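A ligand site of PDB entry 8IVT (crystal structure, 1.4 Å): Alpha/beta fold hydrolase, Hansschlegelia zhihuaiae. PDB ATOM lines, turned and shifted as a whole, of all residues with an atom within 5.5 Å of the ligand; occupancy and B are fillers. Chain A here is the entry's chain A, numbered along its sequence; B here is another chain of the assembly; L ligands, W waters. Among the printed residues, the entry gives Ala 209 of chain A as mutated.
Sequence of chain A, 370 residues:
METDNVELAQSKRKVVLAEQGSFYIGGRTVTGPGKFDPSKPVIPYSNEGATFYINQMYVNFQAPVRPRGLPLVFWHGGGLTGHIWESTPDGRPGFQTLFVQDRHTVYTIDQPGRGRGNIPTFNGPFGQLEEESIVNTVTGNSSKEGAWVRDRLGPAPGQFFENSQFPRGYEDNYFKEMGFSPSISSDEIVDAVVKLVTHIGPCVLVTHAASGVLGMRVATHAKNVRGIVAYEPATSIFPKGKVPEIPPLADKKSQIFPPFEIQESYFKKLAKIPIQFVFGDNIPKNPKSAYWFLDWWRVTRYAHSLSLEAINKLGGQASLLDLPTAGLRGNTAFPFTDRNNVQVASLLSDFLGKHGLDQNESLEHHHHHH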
ATOM      1  N   GLY A  77      -9.425 -21.988  13.508  1.00  0.00           N
ATOM      2  CA  GLY A  77      -8.266 -21.258  13.029  1.00  0.00           C
ATOM      3  C   GLY A  77      -8.254 -19.800  13.450  1.00  0.00           C
ATOM      4  O   GLY A  77      -9.034 -19.349  14.294  1.00  0.00           O
ATOM      5  N   GLY A  78      -7.331 -19.049  12.857  1.00  0.00           N
ATOM      6  CA  GLY A  78      -7.084 -17.685  13.255  1.00  0.00           C
ATOM      7  C   GLY A  78      -8.261 -16.770  13.026  1.00  0.00           C
ATOM      8  O   GLY A  78      -8.828 -16.719  11.922  1.00  0.00           O
ATOM      9  N   GLY A  79      -8.625 -16.003  14.059  1.00  0.00           N
ATOM     10  CA  GLY A  79      -9.706 -15.061  13.929  1.00  0.00           C
ATOM     11  C   GLY A  79     -11.084 -15.663  13.873  1.00  0.00           C
ATOM     12  O   GLY A  79     -12.040 -14.978  13.482  1.00  0.00           O
ATOM     13  N   LEU A  80     -11.238 -16.923  14.279  1.00  0.00           N
ATOM     14  CA  LEU A  80     -12.504 -17.639  14.177  1.00  0.00           C
ATOM     15  C   LEU A  80     -13.001 -18.039  15.558  1.00  0.00           C
ATOM     16  O   LEU A  80     -12.457 -17.649  16.584  1.00  0.00           O
ATOM     17  CB  LEU A  80     -12.329 -18.861  13.266  1.00  0.00           C
ATOM     18  CG  LEU A  80     -11.814 -18.506  11.869  1.00  0.00           C
ATOM     19  CD1 LEU A  80     -11.203 -19.725  11.182  1.00  0.00           C
ATOM     20  CD2 LEU A  80     -12.951 -17.899  11.044  1.00  0.00           C
ATOM     21  N   SER A 142      -7.763  -8.938   9.336  1.00  0.00           N
ATOM     22  CA  SER A 142      -7.891  -9.109   7.904  1.00  0.00           C
ATOM     23  C   SER A 142      -9.148  -8.411   7.389  1.00  0.00           C
ATOM     24  O   SER A 142     -10.132  -8.238   8.104  1.00  0.00           O
ATOM     25  CB  SER A 142      -7.977 -10.592   7.543  1.00  0.00           C
ATOM     26  OG  SER A 142      -7.987 -10.729   6.115  1.00  0.00           O
ATOM     27  N   ARG A 150      -6.670 -15.507   1.150  1.00  0.00           N
ATOM     28  CA  ARG A 150      -6.110 -16.406   2.158  1.00  0.00           C
ATOM     29  C   ARG A 150      -6.783 -17.776   2.131  1.00  0.00           C
ATOM     30  O   ARG A 150      -6.105 -18.805   2.218  1.00  0.00           O
ATOM     31  CB  ARG A 150      -6.290 -15.785   3.547  1.00  0.00           C
ATOM     32  CG  ARG A 150      -5.806 -16.659   4.690  1.00  0.00           C
ATOM     33  CD  ARG A 150      -6.369 -16.161   6.010  1.00  0.00           C
ATOM     34  NE  ARG A 150      -7.810 -16.431   6.119  1.00  0.00           N
ATOM     35  CZ  ARG A 150      -8.601 -15.912   7.060  1.00  0.00           C
ATOM     36  NH1 ARG A 150      -8.108 -15.076   7.972  1.00  0.00           N
ATOM     37  NH2 ARG A 150      -9.882 -16.244   7.088  1.00  0.00           N
ATOM     38  N   ASP A 151      -8.100 -17.799   2.003  1.00  0.00           N
ATOM     39  CA  ASP A 151      -8.841 -19.056   2.066  1.00  0.00           C
ATOM     40  C   ASP A 151      -8.991 -19.724   0.706  1.00  0.00           C
ATOM     41  O   ASP A 151      -9.576 -20.810   0.623  1.00  0.00           O
ATOM     42  CB  ASP A 151     -10.191 -18.806   2.733  1.00  0.00           C
ATOM     43  CG  ASP A 151     -10.030 -18.259   4.155  1.00  0.00           C
ATOM     44  OD1 ASP A 151      -8.934 -18.453   4.719  1.00  0.00           O
ATOM     45  OD2 ASP A 151     -10.976 -17.625   4.682  1.00  0.00           O
ATOM     46  N   HIS A 208      -6.957 -26.290  12.777  1.00  0.00           N
ATOM     47  CA  HIS A 208      -7.249 -25.579  11.542  1.00  0.00           C
ATOM     48  C   HIS A 208      -6.329 -24.371  11.457  1.00  0.00           C
ATOM     49  O   HIS A 208      -6.317 -23.528  12.364  1.00  0.00           O
ATOM     50  CB  HIS A 208      -8.696 -25.079  11.561  1.00  0.00           C
ATOM     51  CG  HIS A 208      -9.045 -24.193  10.407  1.00  0.00           C
ATOM     52  ND1 HIS A 208      -9.737 -23.010  10.556  1.00  0.00           N
ATOM     53  CD2 HIS A 208      -8.812 -24.332   9.083  1.00  0.00           C
ATOM     54  CE1 HIS A 208      -9.921 -22.467   9.364  1.00  0.00           C
ATOM     55  NE2 HIS A 208      -9.361 -23.243   8.451  1.00  0.00           N
ATOM     56  N   ALA A 209      -5.581 -24.275  10.351  1.00  0.00           N
ATOM     57  CA  ALA A 209      -4.866 -23.044  10.057  1.00  0.00           C
ATOM     58  C   ALA A 209      -4.012 -22.589  11.251  1.00  0.00           C
ATOM     59  O   ALA A 209      -3.117 -23.319  11.649  1.00  0.00           O
ATOM     60  CB  ALA A 209      -5.840 -21.952   9.655  1.00  0.00           C
ATOM     61  N   ALA A 210      -4.299 -21.425  11.832  1.00  0.00           N
ATOM     62  CA  ALA A 210      -3.459 -20.918  12.920  1.00  0.00           C
ATOM     63  C   ALA A 210      -3.409 -21.847  14.128  1.00  0.00           C
ATOM     64  O   ALA A 210      -2.456 -21.776  14.905  1.00  0.00           O
ATOM     65  CB  ALA A 210      -3.928 -19.522  13.373  1.00  0.00           C
ATOM     66  N   ALA A 234      -1.129 -23.339   9.395  1.00  0.00           N
ATOM     67  CA  ALA A 234      -0.518 -22.098   8.905  1.00  0.00           C
ATOM     68  C   ALA A 234       0.959 -21.955   9.239  1.00  0.00           C
ATOM     69  O   ALA A 234       1.668 -21.243   8.515  1.00  0.00           O
ATOM     70  CB  ALA A 234      -1.302 -20.874   9.416  1.00  0.00           C
ATOM     71  N   THR A 235       1.445 -22.552  10.329  1.00  0.00           N
ATOM     72  CA  THR A 235       2.850 -22.411  10.725  1.00  0.00           C
ATOM     73  C   THR A 235       3.455 -23.789  10.901  1.00  0.00           C
ATOM     74  O   THR A 235       2.866 -24.643  11.586  1.00  0.00           O
ATOM     75  CB  THR A 235       2.968 -21.597  12.019  1.00  0.00           C
ATOM     76  OG1 THR A 235       2.378 -20.309  11.824  1.00  0.00           O
ATOM     77  CG2 THR A 235       4.446 -21.417  12.426  1.00  0.00           C
ATOM     78  N   PHE A 257       5.506 -17.939   7.207  1.00  0.00           N
ATOM     79  CA  PHE A 257       5.617 -17.676   8.638  1.00  0.00           C
ATOM     80  C   PHE A 257       6.857 -18.375   9.186  1.00  0.00           C
ATOM     81  O   PHE A 257       7.064 -19.553   8.901  1.00  0.00           O
ATOM     82  CB  PHE A 257       4.373 -18.197   9.368  1.00  0.00           C
ATOM     83  CG  PHE A 257       3.134 -17.373   9.153  1.00  0.00           C
ATOM     84  CD1 PHE A 257       3.198 -16.112   8.588  1.00  0.00           C
ATOM     85  CD2 PHE A 257       1.901 -17.888   9.506  1.00  0.00           C
ATOM     86  CE1 PHE A 257       2.039 -15.358   8.396  1.00  0.00           C
ATOM     87  CE2 PHE A 257       0.757 -17.155   9.331  1.00  0.00           C
ATOM     88  CZ  PHE A 257       0.815 -15.889   8.778  1.00  0.00           C
ATOM     89  N   PRO A 258       7.688 -17.684   9.973  1.00  0.00           N
ATOM     90  CA  PRO A 258       8.869 -18.336  10.564  1.00  0.00           C
ATOM     91  C   PRO A 258       8.485 -19.612  11.290  1.00  0.00           C
ATOM     92  O   PRO A 258       7.583 -19.601  12.134  1.00  0.00           O
ATOM     93  CB  PRO A 258       9.388 -17.280  11.538  1.00  0.00           C
ATOM     94  CG  PRO A 258       9.002 -15.974  10.895  1.00  0.00           C
ATOM     95  CD  PRO A 258       7.671 -16.237  10.226  1.00  0.00           C
ATOM     96  N   PHE A 293      -0.996 -15.015  -1.896  1.00  0.00           N
ATOM     97  CA  PHE A 293      -1.438 -16.055  -0.983  1.00  0.00           C
ATOM     98  C   PHE A 293      -1.440 -17.454  -1.595  1.00  0.00           C
ATOM     99  O   PHE A 293      -1.208 -18.423  -0.895  1.00  0.00           O
ATOM    100  CB  PHE A 293      -2.762 -15.704  -0.314  1.00  0.00           C
ATOM    101  CG  PHE A 293      -2.678 -15.644   1.179  1.00  0.00           C
ATOM    102  CD1 PHE A 293      -2.239 -16.747   1.897  1.00  0.00           C
ATOM    103  CD2 PHE A 293      -2.999 -14.493   1.865  1.00  0.00           C
ATOM    104  CE1 PHE A 293      -2.138 -16.701   3.275  1.00  0.00           C
ATOM    105  CE2 PHE A 293      -2.893 -14.438   3.242  1.00  0.00           C
ATOM    106  CZ  PHE A 293      -2.457 -15.540   3.941  1.00  0.00           C
ATOM    107  N   TRP A 296       2.071 -18.333  -1.215  1.00  0.00           N
ATOM    108  CA  TRP A 296       2.346 -18.540   0.198  1.00  0.00           C
ATOM    109  C   TRP A 296       1.954 -19.949   0.571  1.00  0.00           C
ATOM    110  O   TRP A 296       2.713 -20.639   1.237  1.00  0.00           O
ATOM    111  CB  TRP A 296       1.566 -17.531   1.029  1.00  0.00           C
ATOM    112  CG  TRP A 296       1.870 -17.510   2.494  1.00  0.00           C
ATOM    113  CD1 TRP A 296       2.781 -16.731   3.123  1.00  0.00           C
ATOM    114  CD2 TRP A 296       1.219 -18.282   3.509  1.00  0.00           C
ATOM    115  NE1 TRP A 296       2.758 -16.983   4.480  1.00  0.00           N
ATOM    116  CE2 TRP A 296       1.816 -17.930   4.737  1.00  0.00           C
ATOM    117  CE3 TRP A 296       0.209 -19.253   3.502  1.00  0.00           C
ATOM    118  CZ2 TRP A 296       1.418 -18.499   5.939  1.00  0.00           C
ATOM    119  CZ3 TRP A 296      -0.170 -19.810   4.702  1.00  0.00           C
ATOM    120  CH2 TRP A 296       0.433 -19.438   5.900  1.00  0.00           C
ATOM    121  N   TRP A 297       0.774 -20.376   0.151  1.00  0.00           N
ATOM    122  CA  TRP A 297       0.327 -21.732   0.445  1.00  0.00           C
ATOM    123  C   TRP A 297       1.217 -22.778  -0.193  1.00  0.00           C
ATOM    124  O   TRP A 297       1.459 -23.801   0.420  1.00  0.00           O
ATOM    125  CB  TRP A 297      -1.139 -21.918   0.055  1.00  0.00           C
ATOM    126  CG  TRP A 297      -2.090 -21.418   1.082  1.00  0.00           C
ATOM    127  CD1 TRP A 297      -2.950 -20.364   0.954  1.00  0.00           C
ATOM    128  CD2 TRP A 297      -2.282 -21.921   2.408  1.00  0.00           C
ATOM    129  NE1 TRP A 297      -3.659 -20.191   2.103  1.00  0.00           N
ATOM    130  CE2 TRP A 297      -3.272 -21.130   3.013  1.00  0.00           C
ATOM    131  CE3 TRP A 297      -1.714 -22.972   3.140  1.00  0.00           C
ATOM    132  CZ2 TRP A 297      -3.716 -21.355   4.317  1.00  0.00           C
ATOM    133  CZ3 TRP A 297      -2.146 -23.193   4.431  1.00  0.00           C
ATOM    134  CH2 TRP A 297      -3.139 -22.378   5.009  1.00  0.00           C
ATOM    135  N   PHE A 334     -11.086 -23.969   4.282  1.00  0.00           N
ATOM    136  CA  PHE A 334     -12.031 -24.427   5.314  1.00  0.00           C
ATOM    137  C   PHE A 334     -12.782 -25.636   4.763  1.00  0.00           C
ATOM    138  O   PHE A 334     -14.000 -25.559   4.534  1.00  0.00           O
ATOM    139  CB  PHE A 334     -13.073 -23.368   5.682  1.00  0.00           C
ATOM    140  CG  PHE A 334     -12.564 -22.127   6.406  1.00  0.00           C
ATOM    141  CD1 PHE A 334     -11.377 -21.492   6.058  1.00  0.00           C
ATOM    142  CD2 PHE A 334     -13.365 -21.543   7.394  1.00  0.00           C
ATOM    143  CE1 PHE A 334     -10.980 -20.314   6.703  1.00  0.00           C
ATOM    144  CE2 PHE A 334     -12.979 -20.382   8.040  1.00  0.00           C
ATOM    145  CZ  PHE A 334     -11.792 -19.770   7.701  1.00  0.00           C
ATOM    146  N   ILE B  43      -0.142 -10.203   4.310  1.00  0.00           N
ATOM    147  CA  ILE B  43       0.121 -10.158   5.733  1.00  0.00           C
ATOM    148  C   ILE B  43       1.500  -9.519   5.923  1.00  0.00           C
ATOM    149  O   ILE B  43       2.434  -9.872   5.203  1.00  0.00           O
ATOM    150  CB  ILE B  43       0.073 -11.556   6.377  1.00  0.00           C
ATOM    151  CG1 ILE B  43      -1.369 -12.061   6.358  1.00  0.00           C
ATOM    152  CG2 ILE B  43       0.621 -11.529   7.804  1.00  0.00           C
ATOM    153  CD1 ILE B  43      -1.541 -13.493   6.836  1.00  0.00           C
ATOM    154  N   TYR B  45      -1.713  -7.585   7.729  1.00  0.00           N
ATOM    155  CA  TYR B  45      -2.933  -7.108   7.112  1.00  0.00           C
ATOM    156  C   TYR B  45      -2.979  -5.593   7.069  1.00  0.00           C
ATOM    157  O   TYR B  45      -2.452  -4.905   7.945  1.00  0.00           O
ATOM    158  CB  TYR B  45      -4.152  -7.632   7.858  1.00  0.00           C
ATOM    159  CG  TYR B  45      -4.342  -9.116   7.747  1.00  0.00           C
ATOM    160  CD1 TYR B  45      -4.638  -9.695   6.517  1.00  0.00           C
ATOM    161  CD2 TYR B  45      -4.243  -9.949   8.853  1.00  0.00           C
ATOM    162  CE1 TYR B  45      -4.817 -11.058   6.393  1.00  0.00           C
ATOM    163  CE2 TYR B  45      -4.420 -11.313   8.748  1.00  0.00           C
ATOM    164  CZ  TYR B  45      -4.710 -11.860   7.509  1.00  0.00           C
ATOM    165  OH  TYR B  45      -4.902 -13.215   7.357  1.00  0.00           O
HETATM  166  C1  LIG L   1      -2.247 -17.370   7.184  1.00  0.00           C
HETATM  167  C2  LIG L   1      -2.957 -18.527   6.863  1.00  0.00           C
HETATM  168  C3  LIG L   1      -4.114 -18.821   7.584  1.00  0.00           C
HETATM  169  C4  LIG L   1      -4.559 -17.994   8.624  1.00  0.00           C
HETATM  170  C5  LIG L   1      -3.803 -16.770   8.972  1.00  0.00           C
HETATM  171  C6  LIG L   1      -2.664 -16.512   8.211  1.00  0.00           C
HETATM  172  C7  LIG L   1      -5.797 -18.390   9.361  1.00  0.00           C
HETATM  173  O1  LIG L   1      -7.035 -18.149   8.711  1.00  0.00           O
HETATM  174  C8  LIG L   1      -8.246 -18.624   9.287  1.00  0.00           C
HETATM  175  O2  LIG L   1      -5.763 -18.952  10.454  1.00  0.00           O
HETATM  176  S1  LIG L   1      -4.248 -15.719  10.108  1.00  0.00           S
HETATM  177  N1  LIG L   1      -2.917 -14.962  10.537  1.00  0.00           N
HETATM  178  C9  LIG L   1      -2.885 -13.801  11.178  1.00  0.00           C
HETATM  179  O3  LIG L   1      -5.183 -14.842   9.483  1.00  0.00           O
HETATM  180  O4  LIG L   1      -4.853 -16.353  11.237  1.00  0.00           O
HETATM  181  O5  LIG L   1      -3.901 -13.234  11.560  1.00  0.00           O
HETATM  182  N2  LIG L   1      -1.692 -13.259  11.381  1.00  0.00           N
HETATM  183  C10 LIG L   1      -0.606 -14.094  11.691  1.00  0.00           C
HETATM  184  N3  LIG L   1      -0.806 -15.323  12.188  1.00  0.00           N
HETATM  185  C11 LIG L   1       0.233 -16.119  12.497  1.00  0.00           C
HETATM  186  N4  LIG L   1       1.488 -15.660  12.309  1.00  0.00           N
HETATM  187  C12 LIG L   1       1.689 -14.431  11.812  1.00  0.00           C
HETATM  188  N5  LIG L   1       0.642 -13.631  11.514  1.00  0.00           N
HETATM  189  C13 LIG L   1      -1.441 -11.828  11.306  1.00  0.00           C
HETATM  190  O6  LIG L   1       2.959 -13.969  11.632  1.00  0.00           O
HETATM  191  C14 LIG L   1       4.061 -14.800  12.010  1.00  0.00           C
HETATM  192  C15 LIG L   1      -0.019 -17.490  13.043  1.00  0.00           C
HETATM  193  O   HOH W   1      -3.375  -9.150  12.361  1.00  0.00           O
HETATM  194  O   HOH W   2      -3.181 -15.987  13.787  1.00  0.00           O
HETATM  195  O   HOH W   3      -5.311 -10.944  12.313  1.00  0.00           O
HETATM  196  O   HOH W   4      -0.053 -20.580  12.911  1.00  0.00           O
HETATM  197  O   HOH W   5      -0.734 -19.733  15.562  1.00  0.00           O
HETATM  198  O   HOH W   6       2.330 -11.158  10.937  1.00  0.00           O
HETATM  199  O   HOH W   7       5.890 -17.543  12.764  1.00  0.00           O
HETATM  200  O   HOH W   8      -7.053 -13.713  11.489  1.00  0.00           O
HETATM  201  O   HOH W   9       6.974 -15.124  13.719  1.00  0.00           O
HETATM  202  O   HOH W  10       3.335 -18.033  12.932  1.00  0.00           O
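NE of Arg 150 lies close to O1 of the ligand, 3.2 Å away.
An oxygen (O2) of the ligand sits at hydrogen-bond distance from the backbone NH (N) of Ala 210 (3.2 Å).
An oxygen (O3) of the ligand is in hydrogen-bond range of the side-chain hydroxyl (OH) of Tyr 45 of chain B, at 2.7 Å.
O2 of the ligand is in hydrogen-bond range of N of Gly 78, 2.9 Å away.
A ring nitrogen (ND1) of His 208 is in hydrogen-bond range of the backbone NH (N) of Gly 77, at 3.1 Å.
The backbone NH of Ala 234 is in hydrogen-bond range of the backbone carbonyl oxygen of Ala 209 (3.0 Å).
OD1 of Asp 151 is in salt-bridge range of NE of Arg 150 (2.7 Å).
The indole nitrogen of Trp 297 lies within hydrogen-bond range of the backbone carbonyl oxygen of Arg 150 (2.8 Å).
Gly 77 touches the ligand.
Leu 80 touches the ligand.
Ala 209 touches the ligand.
CB of Ala 234 touches C2 of the ligand (3.8 Å).
Thr 235 touches the ligand.
Phe 257 touches the ligand.
CZ of Phe 293 touches C1 of the ligand, 3.7 Å away.
Trp 296 touches the ligand (CH2 to C1, 3.6 Å).
CZ2 of Trp 297 touches C2 of the ligand (3.9 Å).
CD1 of Ile 43 of chain B touches C6 of the ligand (3.5 Å).
14 residues have an atom within 4 Å of the ligand: Gly 77, Gly 78, Leu 80, Arg 150, Ala 209, Ala 210, Ala 234, Thr 235, Phe 257, Phe 293, Trp 296, Trp 297, Ile 43 of chain B and Tyr 45 of chain B.
Along chain A the residues within 4 Å of the ligand span positions 77 to 297.
The nearest printed residue that does not touch the ligand is Phe 334 (4.1 Å).
Water W10 bridges OG1 of Thr 235 (2.7 Å) and N4 of the ligand (3.1 Å).
Water W4 lies within hydrogen-bond range of the side-chain hydroxyl (OG1) of Thr 235 (2.7 Å) and the backbone carbonyl oxygen (O) of Ala 210 (3.3 Å).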
